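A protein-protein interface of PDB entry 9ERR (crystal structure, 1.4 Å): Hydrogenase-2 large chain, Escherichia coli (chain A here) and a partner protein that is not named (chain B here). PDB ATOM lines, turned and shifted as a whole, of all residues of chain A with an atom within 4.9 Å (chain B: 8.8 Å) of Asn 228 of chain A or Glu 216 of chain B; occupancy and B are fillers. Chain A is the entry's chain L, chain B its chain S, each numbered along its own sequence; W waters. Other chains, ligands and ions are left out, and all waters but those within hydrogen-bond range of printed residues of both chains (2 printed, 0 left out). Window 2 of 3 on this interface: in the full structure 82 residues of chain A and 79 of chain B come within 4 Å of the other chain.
The side-chain carboxylate of Glu 216 of chain B sits at hydrogen-bond distance from the side-chain amide nitrogen of Asn 228 of chain A.
The side-chain amide nitrogen of Asn 228 of chain A sits at hydrogen-bond distance from the backbone carbonyl oxygen of Arg 215 of chain B, at 3.0 Å.
The backbone carbonyl oxygen of Ile 227 of chain A sits at hydrogen-bond distance from the guanidinium group of Arg 215 of chain B, 2.7 Å away.
The guanidinium group (NE) of Arg 196 of chain B sits close to the backbone carbonyl oxygen (O) of Gly 217 of chain B (3.4 Å).
A ring nitrogen (ND1) of His 214 of chain B sits at hydrogen-bond distance from the backbone NH (N) of Gly 210 of chain B, 2.8 Å away.
The side-chain carboxylate of Asp 211 of chain B sits at hydrogen-bond distance from the backbone NH of His 214 of chain B (2.8 Å).
OD1 of Asn 228 of chain A is in hydrogen-bond range of N of Gly 231 of chain A.
N of Asp 230 of chain A sits close to OD1 of Asn 228 of chain A (3.0 Å).
N of Asn 228 of chain A is in hydrogen-bond range of O of Leu 235 of chain A.
Among the printed residues, pairs that only touch across the chains: Val 234 of chain A with Gly 217 of chain B, Pro 226 of chain A with His 214 of chain B, Val 234 of chain A with Arg 215 of chain B, Leu 232 of chain A with Glu 216 of chain B, Val 234 of chain A with His 214 of chain B and Pro 226 of chain A with Arg 215 of chain B.
Of the printed residues of chain A, Glu 216 of chain B touches Asn 228 (3.5 Å) and Leu 232 (3.7 Å).
Of the printed residues of chain A, His 214 of chain B touches Pro 226 and Val 234.
Of the printed residues of chain A, Arg 215 of chain B touches Pro 226 (3.7 Å), Ile 227 (2.7 Å), Asn 228 (3.0 Å) and Val 234 (3.6 Å).
Cys 219 of chain B touches none of the printed residues of chain A.
The nearest printed residue of chain A that does not touch Glu 216 of chain B is Val 234 of chain A (4.02 Å).
Of the 10 printed residues of chain A, 5 touch a printed residue of chain B.
Hydrophobic or aromatic side chains of chain A within 4 Å of the printed part of chain B: Pro 226 and Val 234.
Printed residues of chain B that touch a printed residue of chain A: His 214, Arg 215, Glu 216 and Gly 217.
Hydrophobic or aromatic side chains of chain B that line the printed part of chain A: His 214.
Among the printed residues, no Asp or Glu carboxylate lies within 4 Å of a Lys or Arg side-chain nitrogen of the other chain.
Water W1 bridges the side-chain carboxylate of Glu 216 of chain B (2.6 Å) and the side-chain amide nitrogen of Asn 228 of chain A (3.0 Å).
Water W2 bridges the side-chain carboxylate (OE1) of Glu 216 of chain B (2.8 Å) and the backbone NH (N) of Leu 232 of chain A (2.9 Å).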
ATOM      1  N   PRO A 226     -23.705  30.873  -4.195  1.00  0.00           N
ATOM      2  CA  PRO A 226     -24.589  29.709  -4.310  1.00  0.00           C
ATOM      3  C   PRO A 226     -25.927  30.007  -3.655  1.00  0.00           C
ATOM      4  O   PRO A 226     -26.020  30.162  -2.440  1.00  0.00           O
ATOM      5  CB  PRO A 226     -23.801  28.613  -3.564  1.00  0.00           C
ATOM      6  CG  PRO A 226     -22.626  29.303  -2.874  1.00  0.00           C
ATOM      7  CD  PRO A 226     -22.917  30.788  -2.966  1.00  0.00           C
ATOM      8  N   ILE A 227     -26.977  30.173  -4.454  1.00  0.00           N
ATOM      9  CA  ILE A 227     -28.297  30.488  -3.952  1.00  0.00           C
ATOM     10  C   ILE A 227     -28.947  29.192  -3.444  1.00  0.00           C
ATOM     11  O   ILE A 227     -29.176  28.248  -4.209  1.00  0.00           O
ATOM     12  CB  ILE A 227     -29.173  31.194  -4.995  1.00  0.00           C
ATOM     13  CG1 ILE A 227     -28.615  32.592  -5.327  1.00  0.00           C
ATOM     14  CG2 ILE A 227     -30.618  31.276  -4.499  1.00  0.00           C
ATOM     15  CD1 ILE A 227     -29.345  33.316  -6.468  1.00  0.00           C
ATOM     16  N   ASN A 228     -29.262  29.164  -2.149  1.00  0.00           N
ATOM     17  CA  ASN A 228     -29.967  28.027  -1.577  1.00  0.00           C
ATOM     18  C   ASN A 228     -30.588  28.510  -0.268  1.00  0.00           C
ATOM     19  O   ASN A 228     -29.882  28.590   0.753  1.00  0.00           O
ATOM     20  CB  ASN A 228     -29.022  26.853  -1.363  1.00  0.00           C
ATOM     21  CG  ASN A 228     -29.722  25.625  -0.809  1.00  0.00           C
ATOM     22  OD1 ASN A 228     -30.922  25.677  -0.516  1.00  0.00           O
ATOM     23  ND2 ASN A 228     -28.956  24.567  -0.668  1.00  0.00           N
ATOM     24  N   LEU A 229     -31.880  28.826  -0.321  1.00  0.00           N
ATOM     25  CA  LEU A 229     -32.581  29.336   0.860  1.00  0.00           C
ATOM     26  C   LEU A 229     -32.428  28.407   2.062  1.00  0.00           C
ATOM     27  O   LEU A 229     -32.441  28.908   3.198  1.00  0.00           O
ATOM     28  CB  LEU A 229     -34.065  29.539   0.568  1.00  0.00           C
ATOM     29  CG  LEU A 229     -34.432  30.624  -0.430  1.00  0.00           C
ATOM     30  CD1 LEU A 229     -35.931  30.820  -0.507  1.00  0.00           C
ATOM     31  CD2 LEU A 229     -33.784  31.949  -0.067  1.00  0.00           C
ATOM     32  N   ASP A 230     -32.193  27.119   1.809  1.00  0.00           N
ATOM     33  CA  ASP A 230     -32.194  26.102   2.863  1.00  0.00           C
ATOM     34  C   ASP A 230     -30.795  25.552   3.141  1.00  0.00           C
ATOM     35  O   ASP A 230     -30.611  24.602   3.915  1.00  0.00           O
ATOM     36  CB  ASP A 230     -33.177  24.982   2.525  1.00  0.00           C
ATOM     37  CG  ASP A 230     -34.582  25.525   2.484  1.00  0.00           C
ATOM     38  OD1 ASP A 230     -35.098  25.997   3.530  1.00  0.00           O
ATOM     39  OD2 ASP A 230     -35.143  25.545   1.368  1.00  0.00           O
ATOM     40  N   GLY A 231     -29.754  26.203   2.576  1.00  0.00           N
ATOM     41  CA  GLY A 231     -28.416  25.660   2.709  1.00  0.00           C
ATOM     42  C   GLY A 231     -27.638  26.338   3.831  1.00  0.00           C
ATOM     43  O   GLY A 231     -27.720  27.539   3.998  1.00  0.00           O
ATOM     44  N   LEU A 232     -26.866  25.558   4.565  1.00  0.00           N
ATOM     45  CA  LEU A 232     -25.908  26.076   5.524  1.00  0.00           C
ATOM     46  C   LEU A 232     -24.636  26.515   4.792  1.00  0.00           C
ATOM     47  O   LEU A 232     -24.142  25.860   3.870  1.00  0.00           O
ATOM     48  CB  LEU A 232     -25.649  24.967   6.549  1.00  0.00           C
ATOM     49  CG  LEU A 232     -24.787  25.332   7.756  1.00  0.00           C
ATOM     50  CD1 LEU A 232     -25.185  24.495   8.962  1.00  0.00           C
ATOM     51  CD2 LEU A 232     -23.325  25.149   7.450  1.00  0.00           C
ATOM     52  N   VAL A 234     -24.142  29.072   2.671  1.00  0.00           N
ATOM     53  CA  VAL A 234     -24.341  29.611   1.340  1.00  0.00           C
ATOM     54  C   VAL A 234     -25.292  30.799   1.386  1.00  0.00           C
ATOM     55  O   VAL A 234     -25.634  31.283   2.469  1.00  0.00           O
ATOM     56  CB  VAL A 234     -24.802  28.495   0.377  1.00  0.00           C
ATOM     57  CG1 VAL A 234     -23.779  27.380   0.303  1.00  0.00           C
ATOM     58  CG2 VAL A 234     -26.168  27.923   0.705  1.00  0.00           C
ATOM     59  N   LEU A 235     -25.729  31.300   0.222  1.00  0.00           N
ATOM     60  CA  LEU A 235     -26.595  32.475   0.192  1.00  0.00           C
ATOM     61  C   LEU A 235     -28.041  32.047   0.436  1.00  0.00           C
ATOM     62  O   LEU A 235     -28.757  31.634  -0.475  1.00  0.00           O
ATOM     63  CB  LEU A 235     -26.393  33.206  -1.128  1.00  0.00           C
ATOM     64  CG  LEU A 235     -27.158  34.512  -1.299  1.00  0.00           C
ATOM     65  CD1 LEU A 235     -26.783  35.476  -0.207  1.00  0.00           C
ATOM     66  CD2 LEU A 235     -26.851  35.135  -2.635  1.00  0.00           C
ATOM     67  N   ASN A 236     -28.441  32.092   1.712  1.00  0.00           N
ATOM     68  CA  ASN A 236     -29.721  31.611   2.192  1.00  0.00           C
ATOM     69  C   ASN A 236     -30.551  32.811   2.613  1.00  0.00           C
ATOM     70  O   ASN A 236     -30.162  33.971   2.374  1.00  0.00           O
ATOM     71  CB  ASN A 236     -29.553  30.559   3.284  1.00  0.00           C
ATOM     72  CG  ASN A 236     -28.768  31.099   4.466  1.00  0.00           C
ATOM     73  OD1 ASN A 236     -28.858  32.294   4.756  1.00  0.00           O
ATOM     74  ND2 ASN A 236     -28.081  30.236   5.178  1.00  0.00           N
ATOM     75  N   ARG B 196     -13.930  24.738   5.615  1.00  0.00           N
ATOM     76  CA  ARG B 196     -14.340  23.752   4.631  1.00  0.00           C
ATOM     77  C   ARG B 196     -13.357  22.598   4.591  1.00  0.00           C
ATOM     78  O   ARG B 196     -13.565  21.693   3.781  1.00  0.00           O
ATOM     79  CB  ARG B 196     -14.538  24.356   3.241  1.00  0.00           C
ATOM     80  CG  ARG B 196     -15.532  25.512   3.293  1.00  0.00           C
ATOM     81  CD  ARG B 196     -16.084  25.936   1.960  1.00  0.00           C
ATOM     82  NE  ARG B 196     -17.096  26.974   2.140  1.00  0.00           N
ATOM     83  CZ  ARG B 196     -17.992  27.323   1.234  1.00  0.00           C
ATOM     84  NH1 ARG B 196     -17.965  26.780   0.025  1.00  0.00           N
ATOM     85  NH2 ARG B 196     -18.908  28.222   1.532  1.00  0.00           N
ATOM     86  N   HIS B 199     -14.834  19.043   4.356  1.00  0.00           N
ATOM     87  CA  HIS B 199     -15.303  18.694   3.035  1.00  0.00           C
ATOM     88  C   HIS B 199     -14.128  18.238   2.172  1.00  0.00           C
ATOM     89  O   HIS B 199     -14.223  17.201   1.496  1.00  0.00           O
ATOM     90  CB  HIS B 199     -16.058  19.866   2.392  1.00  0.00           C
ATOM     91  CG  HIS B 199     -17.187  20.323   3.242  1.00  0.00           C
ATOM     92  ND1 HIS B 199     -18.162  19.458   3.705  1.00  0.00           N
ATOM     93  CD2 HIS B 199     -17.457  21.520   3.807  1.00  0.00           C
ATOM     94  CE1 HIS B 199     -19.011  20.130   4.442  1.00  0.00           C
ATOM     95  NE2 HIS B 199     -18.609  21.390   4.522  1.00  0.00           N
ATOM     96  N   ARG B 204     -15.636  15.952  -0.623  1.00  0.00           N
ATOM     97  CA  ARG B 204     -16.830  16.724  -0.915  1.00  0.00           C
ATOM     98  C   ARG B 204     -16.437  18.051  -1.559  1.00  0.00           C
ATOM     99  O   ARG B 204     -16.039  18.994  -0.856  1.00  0.00           O
ATOM    100  CB  ARG B 204     -17.647  16.943   0.363  1.00  0.00           C
ATOM    101  CG  ARG B 204     -18.403  15.688   0.825  1.00  0.00           C
ATOM    102  CD  ARG B 204     -19.386  15.941   1.946  1.00  0.00           C
ATOM    103  NE  ARG B 204     -18.788  16.575   3.104  1.00  0.00           N
ATOM    104  CZ  ARG B 204     -18.494  16.004   4.262  1.00  0.00           C
ATOM    105  NH1 ARG B 204     -18.698  14.708   4.469  1.00  0.00           N
ATOM    106  NH2 ARG B 204     -18.052  16.779   5.241  1.00  0.00           N
ATOM    107  N   PHE B 205     -16.548  18.122  -2.910  1.00  0.00           N
ATOM    108  CA  PHE B 205     -16.023  19.237  -3.677  1.00  0.00           C
ATOM    109  C   PHE B 205     -17.083  19.795  -4.623  1.00  0.00           C
ATOM    110  O   PHE B 205     -17.809  19.075  -5.290  1.00  0.00           O
ATOM    111  CB  PHE B 205     -14.837  18.782  -4.530  1.00  0.00           C
ATOM    112  CG  PHE B 205     -13.653  18.252  -3.776  1.00  0.00           C
ATOM    113  CD1 PHE B 205     -12.877  19.082  -2.992  1.00  0.00           C
ATOM    114  CD2 PHE B 205     -13.250  16.928  -3.921  1.00  0.00           C
ATOM    115  CE1 PHE B 205     -11.722  18.641  -2.393  1.00  0.00           C
ATOM    116  CE2 PHE B 205     -12.117  16.478  -3.280  1.00  0.00           C
ATOM    117  CZ  PHE B 205     -11.357  17.309  -2.502  1.00  0.00           C
ATOM    118  N   ALA B 206     -17.166  21.126  -4.675  1.00  0.00           N
ATOM    119  CA  ALA B 206     -17.797  21.816  -5.780  1.00  0.00           C
ATOM    120  C   ALA B 206     -16.981  21.551  -7.042  1.00  0.00           C
ATOM    121  O   ALA B 206     -15.748  21.586  -7.003  1.00  0.00           O
ATOM    122  CB  ALA B 206     -17.862  23.305  -5.508  1.00  0.00           C
ATOM    123  N   GLY B 210     -22.637  26.905  -8.799  1.00  0.00           N
ATOM    124  CA  GLY B 210     -24.045  26.615  -8.941  1.00  0.00           C
ATOM    125  C   GLY B 210     -24.401  25.128  -8.925  1.00  0.00           C
ATOM    126  O   GLY B 210     -25.596  24.819  -8.972  1.00  0.00           O
ATOM    127  N   ASP B 211     -23.411  24.245  -8.827  1.00  0.00           N
ATOM    128  CA  ASP B 211     -23.699  22.808  -8.741  1.00  0.00           C
ATOM    129  C   ASP B 211     -24.130  22.452  -7.314  1.00  0.00           C
ATOM    130  O   ASP B 211     -24.211  23.308  -6.428  1.00  0.00           O
ATOM    131  CB  ASP B 211     -22.570  21.944  -9.283  1.00  0.00           C
ATOM    132  CG  ASP B 211     -21.350  21.686  -8.413  1.00  0.00           C
ATOM    133  OD1 ASP B 211     -21.327  22.146  -7.229  1.00  0.00           O
ATOM    134  OD2 ASP B 211     -20.396  21.027  -8.921  1.00  0.00           O
ATOM    135  N   GLU B 212     -24.512  21.182  -7.108  1.00  0.00           N
ATOM    136  CA  GLU B 212     -25.162  20.848  -5.842  1.00  0.00           C
ATOM    137  C   GLU B 212     -24.181  20.944  -4.678  1.00  0.00           C
ATOM    138  O   GLU B 212     -24.555  21.495  -3.659  1.00  0.00           O
ATOM    139  CB  GLU B 212     -25.765  19.448  -5.912  1.00  0.00           C
ATOM    140  CG  GLU B 212     -27.066  19.488  -6.664  1.00  0.00           C
ATOM    141  CD  GLU B 212     -27.764  18.139  -6.757  1.00  0.00           C
ATOM    142  OE1 GLU B 212     -28.817  18.080  -7.422  1.00  0.00           O
ATOM    143  OE2 GLU B 212     -27.258  17.175  -6.148  1.00  0.00           O
ATOM    144  N   GLY B 213     -22.943  20.497  -4.861  1.00  0.00           N
ATOM    145  CA  GLY B 213     -21.930  20.615  -3.815  1.00  0.00           C
ATOM    146  C   GLY B 213     -21.605  22.074  -3.461  1.00  0.00           C
ATOM    147  O   GLY B 213     -21.518  22.460  -2.280  1.00  0.00           O
ATOM    148  N   HIS B 214     -21.460  22.900  -4.500  1.00  0.00           N
ATOM    149  CA  HIS B 214     -21.281  24.327  -4.327  1.00  0.00           C
ATOM    150  C   HIS B 214     -22.410  24.897  -3.480  1.00  0.00           C
ATOM    151  O   HIS B 214     -22.145  25.704  -2.566  1.00  0.00           O
ATOM    152  CB  HIS B 214     -21.256  24.992  -5.708  1.00  0.00           C
ATOM    153  CG  HIS B 214     -20.831  26.422  -5.669  1.00  0.00           C
ATOM    154  ND1 HIS B 214     -21.651  27.394  -6.179  1.00  0.00           N
ATOM    155  CD2 HIS B 214     -19.715  27.051  -5.177  1.00  0.00           C
ATOM    156  CE1 HIS B 214     -21.045  28.577  -6.027  1.00  0.00           C
ATOM    157  NE2 HIS B 214     -19.911  28.411  -5.381  1.00  0.00           N
ATOM    158  N   ARG B 215     -23.655  24.502  -3.782  1.00  0.00           N
ATOM    159  CA  ARG B 215     -24.822  25.048  -3.106  1.00  0.00           C
ATOM    160  C   ARG B 215     -25.037  24.409  -1.726  1.00  0.00           C
ATOM    161  O   ARG B 215     -25.969  24.784  -1.033  1.00  0.00           O
ATOM    162  CB  ARG B 215     -26.038  24.912  -4.027  1.00  0.00           C
ATOM    163  CG  ARG B 215     -25.959  25.819  -5.249  1.00  0.00           C
ATOM    164  CD  ARG B 215     -27.149  25.657  -6.177  1.00  0.00           C
ATOM    165  NE  ARG B 215     -28.427  26.035  -5.575  1.00  0.00           N
ATOM    166  CZ  ARG B 215     -29.380  25.196  -5.170  1.00  0.00           C
ATOM    167  NH1 ARG B 215     -29.327  23.910  -5.501  1.00  0.00           N
ATOM    168  NH2 ARG B 215     -30.375  25.650  -4.426  1.00  0.00           N
ATOM    169  N   GLU B 216     -24.151  23.495  -1.323  1.00  0.00           N
ATOM    170  CA  GLU B 216     -24.087  22.994   0.039  1.00  0.00           C
ATOM    171  C   GLU B 216     -22.865  23.503   0.817  1.00  0.00           C
ATOM    172  O   GLU B 216     -22.653  23.093   1.968  1.00  0.00           O
ATOM    173  CB  GLU B 216     -24.127  21.460   0.036  1.00  0.00           C
ATOM    174  CG  GLU B 216     -25.487  20.893  -0.398  1.00  0.00           C
ATOM    175  CD  GLU B 216     -26.799  21.338   0.270  1.00  0.00           C
ATOM    176  OE1 GLU B 216     -26.837  21.766   1.470  1.00  0.00           O
ATOM    177  OE2 GLU B 216     -27.859  21.287  -0.416  1.00  0.00           O
ATOM    178  N   GLY B 217     -22.060  24.399   0.233  1.00  0.00           N
ATOM    179  CA  GLY B 217     -20.943  24.978   0.933  1.00  0.00           C
ATOM    180  C   GLY B 217     -19.757  24.028   1.044  1.00  0.00           C
ATOM    181  O   GLY B 217     -18.941  24.152   1.965  1.00  0.00           O
ATOM    182  N   TRP B 218     -19.557  23.187   0.021  1.00  0.00           N
ATOM    183  CA  TRP B 218     -18.464  22.236   0.045  1.00  0.00           C
ATOM    184  C   TRP B 218     -17.148  22.908  -0.333  1.00  0.00           C
ATOM    185  O   TRP B 218     -17.087  24.094  -0.671  1.00  0.00           O
ATOM    186  CB  TRP B 218     -18.761  21.073  -0.910  1.00  0.00           C
ATOM    187  CG  TRP B 218     -19.810  20.123  -0.412  1.00  0.00           C
ATOM    188  CD1 TRP B 218     -20.490  20.149   0.766  1.00  0.00           C
ATOM    189  CD2 TRP B 218     -20.275  18.945  -1.119  1.00  0.00           C
ATOM    190  NE1 TRP B 218     -21.371  19.097   0.827  1.00  0.00           N
ATOM    191  CE2 TRP B 218     -21.248  18.343  -0.311  1.00  0.00           C
ATOM    192  CE3 TRP B 218     -19.946  18.345  -2.341  1.00  0.00           C
ATOM    193  CZ2 TRP B 218     -21.904  17.160  -0.674  1.00  0.00           C
ATOM    194  CZ3 TRP B 218     -20.570  17.168  -2.692  1.00  0.00           C
ATOM    195  CH2 TRP B 218     -21.545  16.585  -1.871  1.00  0.00           C
ATOM    196  N   CYS B 219     -16.058  22.148  -0.241  1.00  0.00           N
ATOM    197  CA  CYS B 219     -14.721  22.672  -0.470  1.00  0.00           C
ATOM    198  C   CYS B 219     -14.559  23.111  -1.930  1.00  0.00           C
ATOM    199  O   CYS B 219     -15.131  22.504  -2.833  1.00  0.00           O
ATOM    200  CB  CYS B 219     -13.667  21.632  -0.094  1.00  0.00           C
ATOM    201  SG  CYS B 219     -11.967  21.964  -0.601  1.00  0.00           S
ATOM    202  N   LEU B 220     -13.783  24.187  -2.140  1.00  0.00           N
ATOM    203  CA  LEU B 220     -13.608  24.813  -3.440  1.00  0.00           C
ATOM    204  C   LEU B 220     -12.260  24.469  -4.077  1.00  0.00           C
ATOM    205  O   LEU B 220     -11.845  25.112  -5.046  1.00  0.00           O
ATOM    206  CB  LEU B 220     -13.816  26.334  -3.286  1.00  0.00           C
ATOM    207  CG  LEU B 220     -15.111  26.757  -2.598  1.00  0.00           C
ATOM    208  CD1 LEU B 220     -15.233  28.291  -2.606  1.00  0.00           C
ATOM    209  CD2 LEU B 220     -16.321  26.135  -3.238  1.00  0.00           C
ATOM    210  N   ALA B 249     -16.267  31.728   1.762  1.00  0.00           N
ATOM    211  CA  ALA B 249     -17.586  31.630   2.380  1.00  0.00           C
ATOM    212  C   ALA B 249     -18.667  32.143   1.420  1.00  0.00           C
ATOM    213  O   ALA B 249     -19.806  31.703   1.492  1.00  0.00           O
ATOM    214  CB  ALA B 249     -17.628  32.375   3.684  1.00  0.00           C
HETATM  215  O   HOH W   1     -30.115  22.130   0.659  1.00  0.00           O
HETATM  216  O   HOH W   2     -25.516  23.260   3.433  1.00  0.00           O
